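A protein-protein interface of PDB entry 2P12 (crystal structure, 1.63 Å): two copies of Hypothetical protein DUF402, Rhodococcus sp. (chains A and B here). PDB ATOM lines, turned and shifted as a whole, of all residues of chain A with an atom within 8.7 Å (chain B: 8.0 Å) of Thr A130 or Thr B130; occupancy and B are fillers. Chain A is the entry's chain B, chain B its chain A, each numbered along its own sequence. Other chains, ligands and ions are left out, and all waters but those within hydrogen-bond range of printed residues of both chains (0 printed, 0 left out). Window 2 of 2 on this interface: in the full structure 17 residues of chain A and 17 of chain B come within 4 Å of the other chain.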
ATOM      1  N   ASP A 123     -22.510 -22.462  12.229  1.00  0.00           N
ATOM      2  CA  ASP A 123     -21.505 -23.450  11.830  1.00  0.00           C
ATOM      3  C   ASP A 123     -22.034 -24.878  11.982  1.00  0.00           C
ATOM      4  O   ASP A 123     -21.819 -25.707  11.103  1.00  0.00           O
ATOM      5  CB  ASP A 123     -20.164 -23.228  12.551  1.00  0.00           C
ATOM      6  CG  ASP A 123     -20.268 -23.225  14.071  1.00  0.00           C
ATOM      7  OD1 ASP A 123     -21.355 -23.104  14.673  1.00  0.00           O
ATOM      8  OD2 ASP A 123     -19.196 -23.338  14.711  1.00  0.00           O
ATOM      9  N   GLU A 124     -22.744 -25.132  13.082  1.00  0.00           N
ATOM     10  CA  GLU A 124     -23.348 -26.447  13.361  1.00  0.00           C
ATOM     11  C   GLU A 124     -24.376 -26.814  12.301  1.00  0.00           C
ATOM     12  O   GLU A 124     -24.398 -27.943  11.855  1.00  0.00           O
ATOM     13  CB  GLU A 124     -24.002 -26.462  14.741  1.00  0.00           C
ATOM     14  CG  GLU A 124     -23.050 -26.776  15.885  1.00  0.00           C
ATOM     15  CD  GLU A 124     -23.753 -26.806  17.231  1.00  0.00           C
ATOM     16  OE1 GLU A 124     -25.001 -26.714  17.279  1.00  0.00           O
ATOM     17  OE2 GLU A 124     -23.056 -26.923  18.261  1.00  0.00           O
ATOM     18  N   LEU A 125     -25.248 -25.866  11.930  1.00  0.00           N
ATOM     19  CA  LEU A 125     -26.194 -26.055  10.814  1.00  0.00           C
ATOM     20  C   LEU A 125     -25.460 -26.382   9.494  1.00  0.00           C
ATOM     21  O   LEU A 125     -25.848 -27.312   8.766  1.00  0.00           O
ATOM     22  CB  LEU A 125     -27.120 -24.828  10.633  1.00  0.00           C
ATOM     23  CG  LEU A 125     -28.150 -24.939   9.494  1.00  0.00           C
ATOM     24  CD1 LEU A 125     -29.175 -26.088   9.764  1.00  0.00           C
ATOM     25  CD2 LEU A 125     -28.889 -23.635   9.227  1.00  0.00           C
ATOM     26  N   MET A 126     -24.394 -25.628   9.203  1.00  0.00           N
ATOM     27  CA  MET A 126     -23.621 -25.844   7.976  1.00  0.00           C
ATOM     28  C   MET A 126     -23.071 -27.280   7.970  1.00  0.00           C
ATOM     29  O   MET A 126     -23.185 -27.966   6.950  1.00  0.00           O
ATOM     30  CB  MET A 126     -22.482 -24.807   7.806  1.00  0.00           C
ATOM     31  CG  MET A 126     -22.917 -23.324   7.472  1.00  0.00           C
ATOM     32  SD  MET A 126     -24.428 -23.102   6.209  1.00  0.00           S
ATOM     33  CE  MET A 126     -23.531 -23.499   4.583  1.00  0.00           C
ATOM     34  N   GLU A 127     -22.502 -27.734   9.087  1.00  0.00           N
ATOM     35  CA  GLU A 127     -21.890 -29.085   9.157  1.00  0.00           C
ATOM     36  C   GLU A 127     -22.923 -30.226   9.136  1.00  0.00           C
ATOM     37  O   GLU A 127     -22.628 -31.319   8.638  1.00  0.00           O
ATOM     38  CB  GLU A 127     -20.952 -29.208  10.371  1.00  0.00           C
ATOM     39  CG  GLU A 127     -20.388 -30.622  10.672  1.00  0.00           C
ATOM     40  CD  GLU A 127     -19.261 -31.057   9.733  1.00  0.00           C
ATOM     41  OE1 GLU A 127     -18.704 -30.198   9.006  1.00  0.00           O
ATOM     42  OE2 GLU A 127     -18.918 -32.270   9.731  1.00  0.00           O
ATOM     43  N   ALA A 128     -24.116 -29.977   9.681  1.00  0.00           N
ATOM     44  CA  ALA A 128     -25.221 -30.930   9.587  1.00  0.00           C
ATOM     45  C   ALA A 128     -25.747 -31.031   8.168  1.00  0.00           C
ATOM     46  O   ALA A 128     -26.014 -32.121   7.688  1.00  0.00           O
ATOM     47  CB  ALA A 128     -26.339 -30.573  10.534  1.00  0.00           C
ATOM     48  N   HIS A 129     -25.859 -29.904   7.471  1.00  0.00           N
ATOM     49  CA  HIS A 129     -26.323 -29.934   6.086  1.00  0.00           C
ATOM     50  C   HIS A 129     -25.336 -30.652   5.172  1.00  0.00           C
ATOM     51  O   HIS A 129     -25.729 -31.503   4.345  1.00  0.00           O
ATOM     52  CB  HIS A 129     -26.540 -28.520   5.569  1.00  0.00           C
ATOM     53  CG  HIS A 129     -26.936 -28.470   4.136  1.00  0.00           C
ATOM     54  ND1 HIS A 129     -28.217 -28.732   3.705  1.00  0.00           N
ATOM     55  CD2 HIS A 129     -26.212 -28.200   3.025  1.00  0.00           C
ATOM     56  CE1 HIS A 129     -28.261 -28.626   2.388  1.00  0.00           C
ATOM     57  NE2 HIS A 129     -27.063 -28.296   1.955  1.00  0.00           N
ATOM     58  N   THR A 130     -24.055 -30.316   5.310  1.00  0.00           N
ATOM     59  CA  THR A 130     -23.073 -30.850   4.374  1.00  0.00           C
ATOM     60  C   THR A 130     -22.892 -32.377   4.561  1.00  0.00           C
ATOM     61  O   THR A 130     -22.634 -33.102   3.592  1.00  0.00           O
ATOM     62  CB  THR A 130     -21.727 -30.042   4.367  1.00  0.00           C
ATOM     63  OG1 THR A 130     -20.991 -30.343   3.159  1.00  0.00           O
ATOM     64  CG2 THR A 130     -20.858 -30.364   5.589  1.00  0.00           C
ATOM     65  N   THR A 131     -23.065 -32.847   5.800  1.00  0.00           N
ATOM     66  CA  THR A 131     -22.915 -34.276   6.118  1.00  0.00           C
ATOM     67  C   THR A 131     -24.208 -35.082   5.975  1.00  0.00           C
ATOM     68  O   THR A 131     -24.228 -36.285   6.263  1.00  0.00           O
ATOM     69  CB  THR A 131     -22.325 -34.514   7.528  1.00  0.00           C
ATOM     70  OG1 THR A 131     -23.224 -34.022   8.521  1.00  0.00           O
ATOM     71  CG2 THR A 131     -20.949 -33.870   7.680  1.00  0.00           C
ATOM     72  N   GLY A 132     -25.271 -34.432   5.519  1.00  0.00           N
ATOM     73  CA  GLY A 132     -26.522 -35.108   5.206  1.00  0.00           C
ATOM     74  C   GLY A 132     -27.474 -35.348   6.371  1.00  0.00           C
ATOM     75  O   GLY A 132     -28.436 -36.100   6.227  1.00  0.00           O
ATOM     76  N   LEU A 133     -27.230 -34.724   7.521  1.00  0.00           N
ATOM     77  CA  LEU A 133     -28.115 -34.930   8.682  1.00  0.00           C
ATOM     78  C   LEU A 133     -29.447 -34.177   8.528  1.00  0.00           C
ATOM     79  O   LEU A 133     -30.407 -34.453   9.232  1.00  0.00           O
ATOM     80  CB  LEU A 133     -27.419 -34.571  10.005  1.00  0.00           C
ATOM     81  CG  LEU A 133     -26.000 -35.105  10.239  1.00  0.00           C
ATOM     82  CD1 LEU A 133     -25.500 -34.668  11.609  1.00  0.00           C
ATOM     83  CD2 LEU A 133     -25.939 -36.620  10.110  1.00  0.00           C
ATOM     84  N   LEU A 134     -29.492 -33.197   7.629  1.00  0.00           N
ATOM     85  CA  LEU A 134     -30.762 -32.571   7.244  1.00  0.00           C
ATOM     86  C   LEU A 134     -30.654 -32.003   5.846  1.00  0.00           C
ATOM     87  O   LEU A 134     -29.553 -31.675   5.375  1.00  0.00           O
ATOM     88  CB  LEU A 134     -31.253 -31.537   8.270  1.00  0.00           C
ATOM     89  CG  LEU A 134     -30.329 -30.583   9.043  1.00  0.00           C
ATOM     90  CD1 LEU A 134     -29.309 -29.995   8.118  1.00  0.00           C
ATOM     91  CD2 LEU A 134     -31.126 -29.497   9.756  1.00  0.00           C
ATOM     92  N   ASP A 135     -31.777 -31.913   5.153  1.00  0.00           N
ATOM     93  CA  ASP A 135     -31.709 -31.560   3.742  1.00  0.00           C
ATOM     94  C   ASP A 135     -31.692 -30.040   3.551  1.00  0.00           C
ATOM     95  O   ASP A 135     -31.791 -29.282   4.529  1.00  0.00           O
ATOM     96  CB  ASP A 135     -32.823 -32.247   2.938  1.00  0.00           C
ATOM     97  CG  ASP A 135     -34.209 -31.956   3.471  1.00  0.00           C
ATOM     98  OD1 ASP A 135     -34.442 -30.871   4.044  1.00  0.00           O
ATOM     99  OD2 ASP A 135     -35.094 -32.820   3.308  1.00  0.00           O
ATOM    100  N   THR A 136     -31.568 -29.601   2.301  1.00  0.00           N
ATOM    101  CA  THR A 136     -31.487 -28.178   1.996  1.00  0.00           C
ATOM    102  C   THR A 136     -32.762 -27.486   2.362  1.00  0.00           C
ATOM    103  O   THR A 136     -32.714 -26.391   2.919  1.00  0.00           O
ATOM    104  CB  THR A 136     -31.170 -27.929   0.503  1.00  0.00           C
ATOM    105  OG1 THR A 136     -30.043 -28.731   0.149  1.00  0.00           O
ATOM    106  CG2 THR A 136     -30.882 -26.464   0.255  1.00  0.00           C
ATOM    107  N   ALA A 139     -32.675 -26.953   6.116  1.00  0.00           N
ATOM    108  CA  ALA A 139     -31.657 -25.938   6.430  1.00  0.00           C
ATOM    109  C   ALA A 139     -32.195 -24.577   6.038  1.00  0.00           C
ATOM    110  O   ALA A 139     -32.144 -23.603   6.811  1.00  0.00           O
ATOM    111  CB  ALA A 139     -30.310 -26.238   5.709  1.00  0.00           C
ATOM    112  N   ILE B  10     -24.358 -23.879  -7.466  1.00  0.00           N
ATOM    113  CA  ILE B  10     -24.586 -23.838  -8.956  1.00  0.00           C
ATOM    114  C   ILE B  10     -23.333 -23.315  -9.708  1.00  0.00           C
ATOM    115  O   ILE B  10     -22.472 -24.104 -10.062  1.00  0.00           O
ATOM    116  CB  ILE B  10     -25.916 -23.049  -9.296  1.00  0.00           C
ATOM    117  CG1 ILE B  10     -26.218 -23.065 -10.831  1.00  0.00           C
ATOM    118  CG2 ILE B  10     -25.989 -21.693  -8.506  1.00  0.00           C
ATOM    119  CD1 ILE B  10     -25.828 -21.800 -11.659  1.00  0.00           C
ATOM    120  N   ASP B 123     -31.153 -21.127  -0.751  1.00  0.00           N
ATOM    121  CA  ASP B 123     -30.935 -22.427  -1.409  1.00  0.00           C
ATOM    122  C   ASP B 123     -29.639 -22.466  -2.207  1.00  0.00           C
ATOM    123  O   ASP B 123     -28.912 -23.452  -2.159  1.00  0.00           O
ATOM    124  CB  ASP B 123     -32.161 -22.866  -2.258  1.00  0.00           C
ATOM    125  CG  ASP B 123     -32.505 -21.876  -3.398  1.00  0.00           C
ATOM    126  OD1 ASP B 123     -32.144 -20.675  -3.339  1.00  0.00           O
ATOM    127  OD2 ASP B 123     -33.172 -22.307  -4.366  1.00  0.00           O
ATOM    128  N   GLU B 124     -29.317 -21.377  -2.900  1.00  0.00           N
ATOM    129  CA  GLU B 124     -28.083 -21.322  -3.673  1.00  0.00           C
ATOM    130  C   GLU B 124     -26.868 -21.349  -2.774  1.00  0.00           C
ATOM    131  O   GLU B 124     -25.899 -22.021  -3.074  1.00  0.00           O
ATOM    132  CB  GLU B 124     -28.045 -20.099  -4.581  1.00  0.00           C
ATOM    133  CG  GLU B 124     -29.255 -19.998  -5.476  1.00  0.00           C
ATOM    134  CD  GLU B 124     -29.054 -19.124  -6.694  1.00  0.00           C
ATOM    135  OE1 GLU B 124     -28.159 -18.253  -6.715  1.00  0.00           O
ATOM    136  OE2 GLU B 124     -29.813 -19.326  -7.665  1.00  0.00           O
ATOM    137  N   LEU B 125     -26.915 -20.626  -1.656  1.00  0.00           N
ATOM    138  CA  LEU B 125     -25.776 -20.653  -0.723  1.00  0.00           C
ATOM    139  C   LEU B 125     -25.529 -22.072  -0.221  1.00  0.00           C
ATOM    140  O   LEU B 125     -24.374 -22.551  -0.145  1.00  0.00           O
ATOM    141  CB  LEU B 125     -26.054 -19.715   0.462  1.00  0.00           C
ATOM    142  CG  LEU B 125     -24.925 -19.720   1.491  1.00  0.00           C
ATOM    143  CD1 LEU B 125     -23.581 -19.204   0.955  1.00  0.00           C
ATOM    144  CD2 LEU B 125     -25.351 -18.922   2.736  1.00  0.00           C
ATOM    145  N   MET B 126     -26.631 -22.725   0.154  1.00  0.00           N
ATOM    146  CA  MET B 126     -26.582 -24.114   0.632  1.00  0.00           C
ATOM    147  C   MET B 126     -25.929 -25.018  -0.410  1.00  0.00           C
ATOM    148  O   MET B 126     -24.995 -25.761  -0.053  1.00  0.00           O
ATOM    149  CB  MET B 126     -27.956 -24.640   1.101  1.00  0.00           C
ATOM    150  CG  MET B 126     -28.616 -23.942   2.310  1.00  0.00           C
ATOM    151  SD  MET B 126     -27.412 -23.506   3.772  1.00  0.00           S
ATOM    152  CE  MET B 126     -26.997 -25.263   4.377  1.00  0.00           C
ATOM    153  N   GLU B 127     -26.372 -24.958  -1.661  1.00  0.00           N
ATOM    154  CA  GLU B 127     -25.810 -25.856  -2.684  1.00  0.00           C
ATOM    155  C   GLU B 127     -24.354 -25.505  -3.043  1.00  0.00           C
ATOM    156  O   GLU B 127     -23.569 -26.398  -3.354  1.00  0.00           O
ATOM    157  CB  GLU B 127     -26.703 -25.876  -3.914  1.00  0.00           C
ATOM    158  CG  GLU B 127     -26.190 -26.753  -5.041  1.00  0.00           C
ATOM    159  CD  GLU B 127     -27.099 -26.748  -6.249  1.00  0.00           C
ATOM    160  OE1 GLU B 127     -27.866 -25.777  -6.429  1.00  0.00           O
ATOM    161  OE2 GLU B 127     -27.034 -27.718  -7.026  1.00  0.00           O
ATOM    162  N   ALA B 128     -23.985 -24.221  -3.009  1.00  0.00           N
ATOM    163  CA  ALA B 128     -22.576 -23.847  -3.211  1.00  0.00           C
ATOM    164  C   ALA B 128     -21.686 -24.376  -2.099  1.00  0.00           C
ATOM    165  O   ALA B 128     -20.549 -24.813  -2.340  1.00  0.00           O
ATOM    166  CB  ALA B 128     -22.420 -22.294  -3.340  1.00  0.00           C
ATOM    167  N   HIS B 129     -22.200 -24.358  -0.884  1.00  0.00           N
ATOM    168  CA  HIS B 129     -21.453 -24.867   0.237  1.00  0.00           C
ATOM    169  C   HIS B 129     -21.310 -26.383   0.145  1.00  0.00           C
ATOM    170  O   HIS B 129     -20.217 -26.913   0.382  1.00  0.00           O
ATOM    171  CB  HIS B 129     -22.122 -24.506   1.561  1.00  0.00           C
ATOM    172  CG  HIS B 129     -21.387 -25.047   2.748  1.00  0.00           C
ATOM    173  ND1 HIS B 129     -20.087 -24.687   3.039  1.00  0.00           N
ATOM    174  CD2 HIS B 129     -21.754 -25.936   3.697  1.00  0.00           C
ATOM    175  CE1 HIS B 129     -19.697 -25.320   4.131  1.00  0.00           C
ATOM    176  NE2 HIS B 129     -20.691 -26.075   4.552  1.00  0.00           N
ATOM    177  N   THR B 130     -22.387 -27.089  -0.195  1.00  0.00           N
ATOM    178  CA  THR B 130     -22.276 -28.560  -0.183  1.00  0.00           C
ATOM    179  C   THR B 130     -21.363 -29.032  -1.285  1.00  0.00           C
ATOM    180  O   THR B 130     -20.719 -30.086  -1.149  1.00  0.00           O
ATOM    181  CB  THR B 130     -23.630 -29.323  -0.254  1.00  0.00           C
ATOM    182  OG1 THR B 130     -24.391 -28.892  -1.389  1.00  0.00           O
ATOM    183  CG2 THR B 130     -24.421 -29.088   0.963  1.00  0.00           C
ATOM    184  N   THR B 131     -21.296 -28.279  -2.378  1.00  0.00           N
ATOM    185  CA  THR B 131     -20.483 -28.710  -3.519  1.00  0.00           C
ATOM    186  C   THR B 131     -19.065 -28.118  -3.451  1.00  0.00           C
ATOM    187  O   THR B 131     -18.252 -28.342  -4.343  1.00  0.00           O
ATOM    188  CB  THR B 131     -21.150 -28.345  -4.851  1.00  0.00           C
ATOM    189  OG1 THR B 131     -21.353 -26.938  -4.883  1.00  0.00           O
ATOM    190  CG2 THR B 131     -22.510 -29.037  -4.995  1.00  0.00           C
ATOM    191  N   GLY B 132     -18.785 -27.360  -2.391  1.00  0.00           N
ATOM    192  CA  GLY B 132     -17.431 -26.884  -2.114  1.00  0.00           C
ATOM    193  C   GLY B 132     -16.995 -25.670  -2.912  1.00  0.00           C
ATOM    194  O   GLY B 132     -15.796 -25.447  -3.088  1.00  0.00           O
ATOM    195  N   LEU B 133     -17.961 -24.898  -3.401  1.00  0.00           N
ATOM    196  CA  LEU B 133     -17.661 -23.668  -4.154  1.00  0.00           C
ATOM    197  C   LEU B 133     -17.291 -22.499  -3.245  1.00  0.00           C
ATOM    198  O   LEU B 133     -16.644 -21.547  -3.688  1.00  0.00           O
ATOM    199  CB  LEU B 133     -18.789 -23.288  -5.092  1.00  0.00           C
ATOM    200  CG  LEU B 133     -19.197 -24.348  -6.107  1.00  0.00           C
ATOM    201  CD1 LEU B 133     -20.325 -23.851  -6.954  1.00  0.00           C
ATOM    202  CD2 LEU B 133     -18.000 -24.842  -6.956  1.00  0.00           C
ATOM    203  N   LEU B 134     -17.715 -22.563  -1.982  1.00  0.00           N
ATOM    204  CA  LEU B 134     -17.130 -21.710  -0.941  1.00  0.00           C
ATOM    205  C   LEU B 134     -17.042 -22.465   0.374  1.00  0.00           C
ATOM    206  O   LEU B 134     -17.812 -23.402   0.625  1.00  0.00           O
ATOM    207  CB  LEU B 134     -17.905 -20.398  -0.747  1.00  0.00           C
ATOM    208  CG  LEU B 134     -19.421 -20.339  -0.898  1.00  0.00           C
ATOM    209  CD1 LEU B 134     -20.132 -21.435  -0.169  1.00  0.00           C
ATOM    210  CD2 LEU B 134     -19.927 -18.986  -0.410  1.00  0.00           C
ATOM    211  N   THR B 136     -16.928 -23.183   4.664  1.00  0.00           N
ATOM    212  CA  THR B 136     -17.895 -23.035   5.756  1.00  0.00           C
ATOM    213  C   THR B 136     -17.782 -21.677   6.419  1.00  0.00           C
ATOM    214  O   THR B 136     -18.805 -21.064   6.711  1.00  0.00           O
ATOM    215  CB  THR B 136     -17.778 -24.150   6.827  1.00  0.00           C
ATOM    216  OG1 THR B 136     -17.686 -25.420   6.175  1.00  0.00           O
ATOM    217  CG2 THR B 136     -18.990 -24.156   7.752  1.00  0.00           C
ATOM    218  N   ALA B 139     -19.484 -19.227   4.070  1.00  0.00           N
ATOM    219  CA  ALA B 139     -20.929 -19.392   4.068  1.00  0.00           C
ATOM    220  C   ALA B 139     -21.532 -18.883   5.376  1.00  0.00           C
ATOM    221  O   ALA B 139     -22.540 -18.156   5.367  1.00  0.00           O
ATOM    222  CB  ALA B 139     -21.330 -20.835   3.748  1.00  0.00           C
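The backbone carbonyl oxygen (O) of Met B126 is in hydrogen-bond range of the side-chain hydroxyl (OG1) of Thr B130, at 3.5 Å.
The backbone carbonyl oxygen of Glu B127 is in hydrogen-bond range of the side-chain hydroxyl of Thr B130, 3.3 Å away.
OG1 of Thr B136 sits close to NE2 of His B129, 3.5 Å away.
Among the printed residues, pairs that only touch across the chains: Met A126 with Met B126, Met A126 with His B129, Met A126 with Thr B136, Met A126 with Ala B139, His A129 with Met B126, His A129 with Thr B130, Thr A130 with Thr B130, Thr A136 with Met B126 and Ala A139 with Met B126.
Of the printed residues of chain B, Thr A130 touches Thr B130.
Of the printed residues of chain A, Thr B130 touches His A129 and Thr A130.
No residue of chain A comes within 4 Å of Thr B131.
Of the printed residues of chain A, Thr B136 touches Met A126 (3.6 Å).
Printed residues of chain B within 4 Å of Thr A136: Met B126 (3.6 Å).
Of the printed residues of chain A, Met B126 touches Met A126, His A129, Thr A136 and Ala A139.
Printed residues of chain A within 4 Å of Ala B139: Met A126 (3.6 Å).
Of the printed residues of chain A, His B129 touches Met A126.
Glu B127 touches none of the printed residues of chain A.
Asp A123 touches none of the printed residues of chain B.
The nearest printed residue of chain A that does not touch Thr B130 is Thr A136 (5.7 Å).
The nearest printed residue of chain A that does not touch Met B126 is Leu A125 (5.0 Å).
Of the 15 printed residues of chain A, 5 touch a printed residue of chain B.
Printed residues of chain A that touch a printed residue of chain B: Met A126, His A129, Thr A130, Thr A136 and Ala A139.
Of the 15 printed residues of chain B, 5 touch a printed residue of chain A.
Among the printed residues, no Asp or Glu carboxylate lies within 4 Å of a Lys or Arg side-chain nitrogen of the other chain.
Met B126 touches its own counterpart, Met A126.
Met A126 touches His B129, and with the chains exchanged His A129 touches Met B126.
Met A126 touches Thr B136, and with the chains exchanged Thr A136 touches Met B126.
Met A126 touches Ala B139, and with the chains exchanged Ala A139 touches Met B126.
Positions printed for both chains: 123, 124, 125, 126, 127, 128, 129, 130, 131, 132, 133, 134, 136 and 139.
Of the 9 pairs that touch across the chains among the printed residues, 8 have their exchanged pair printed and touching as well.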
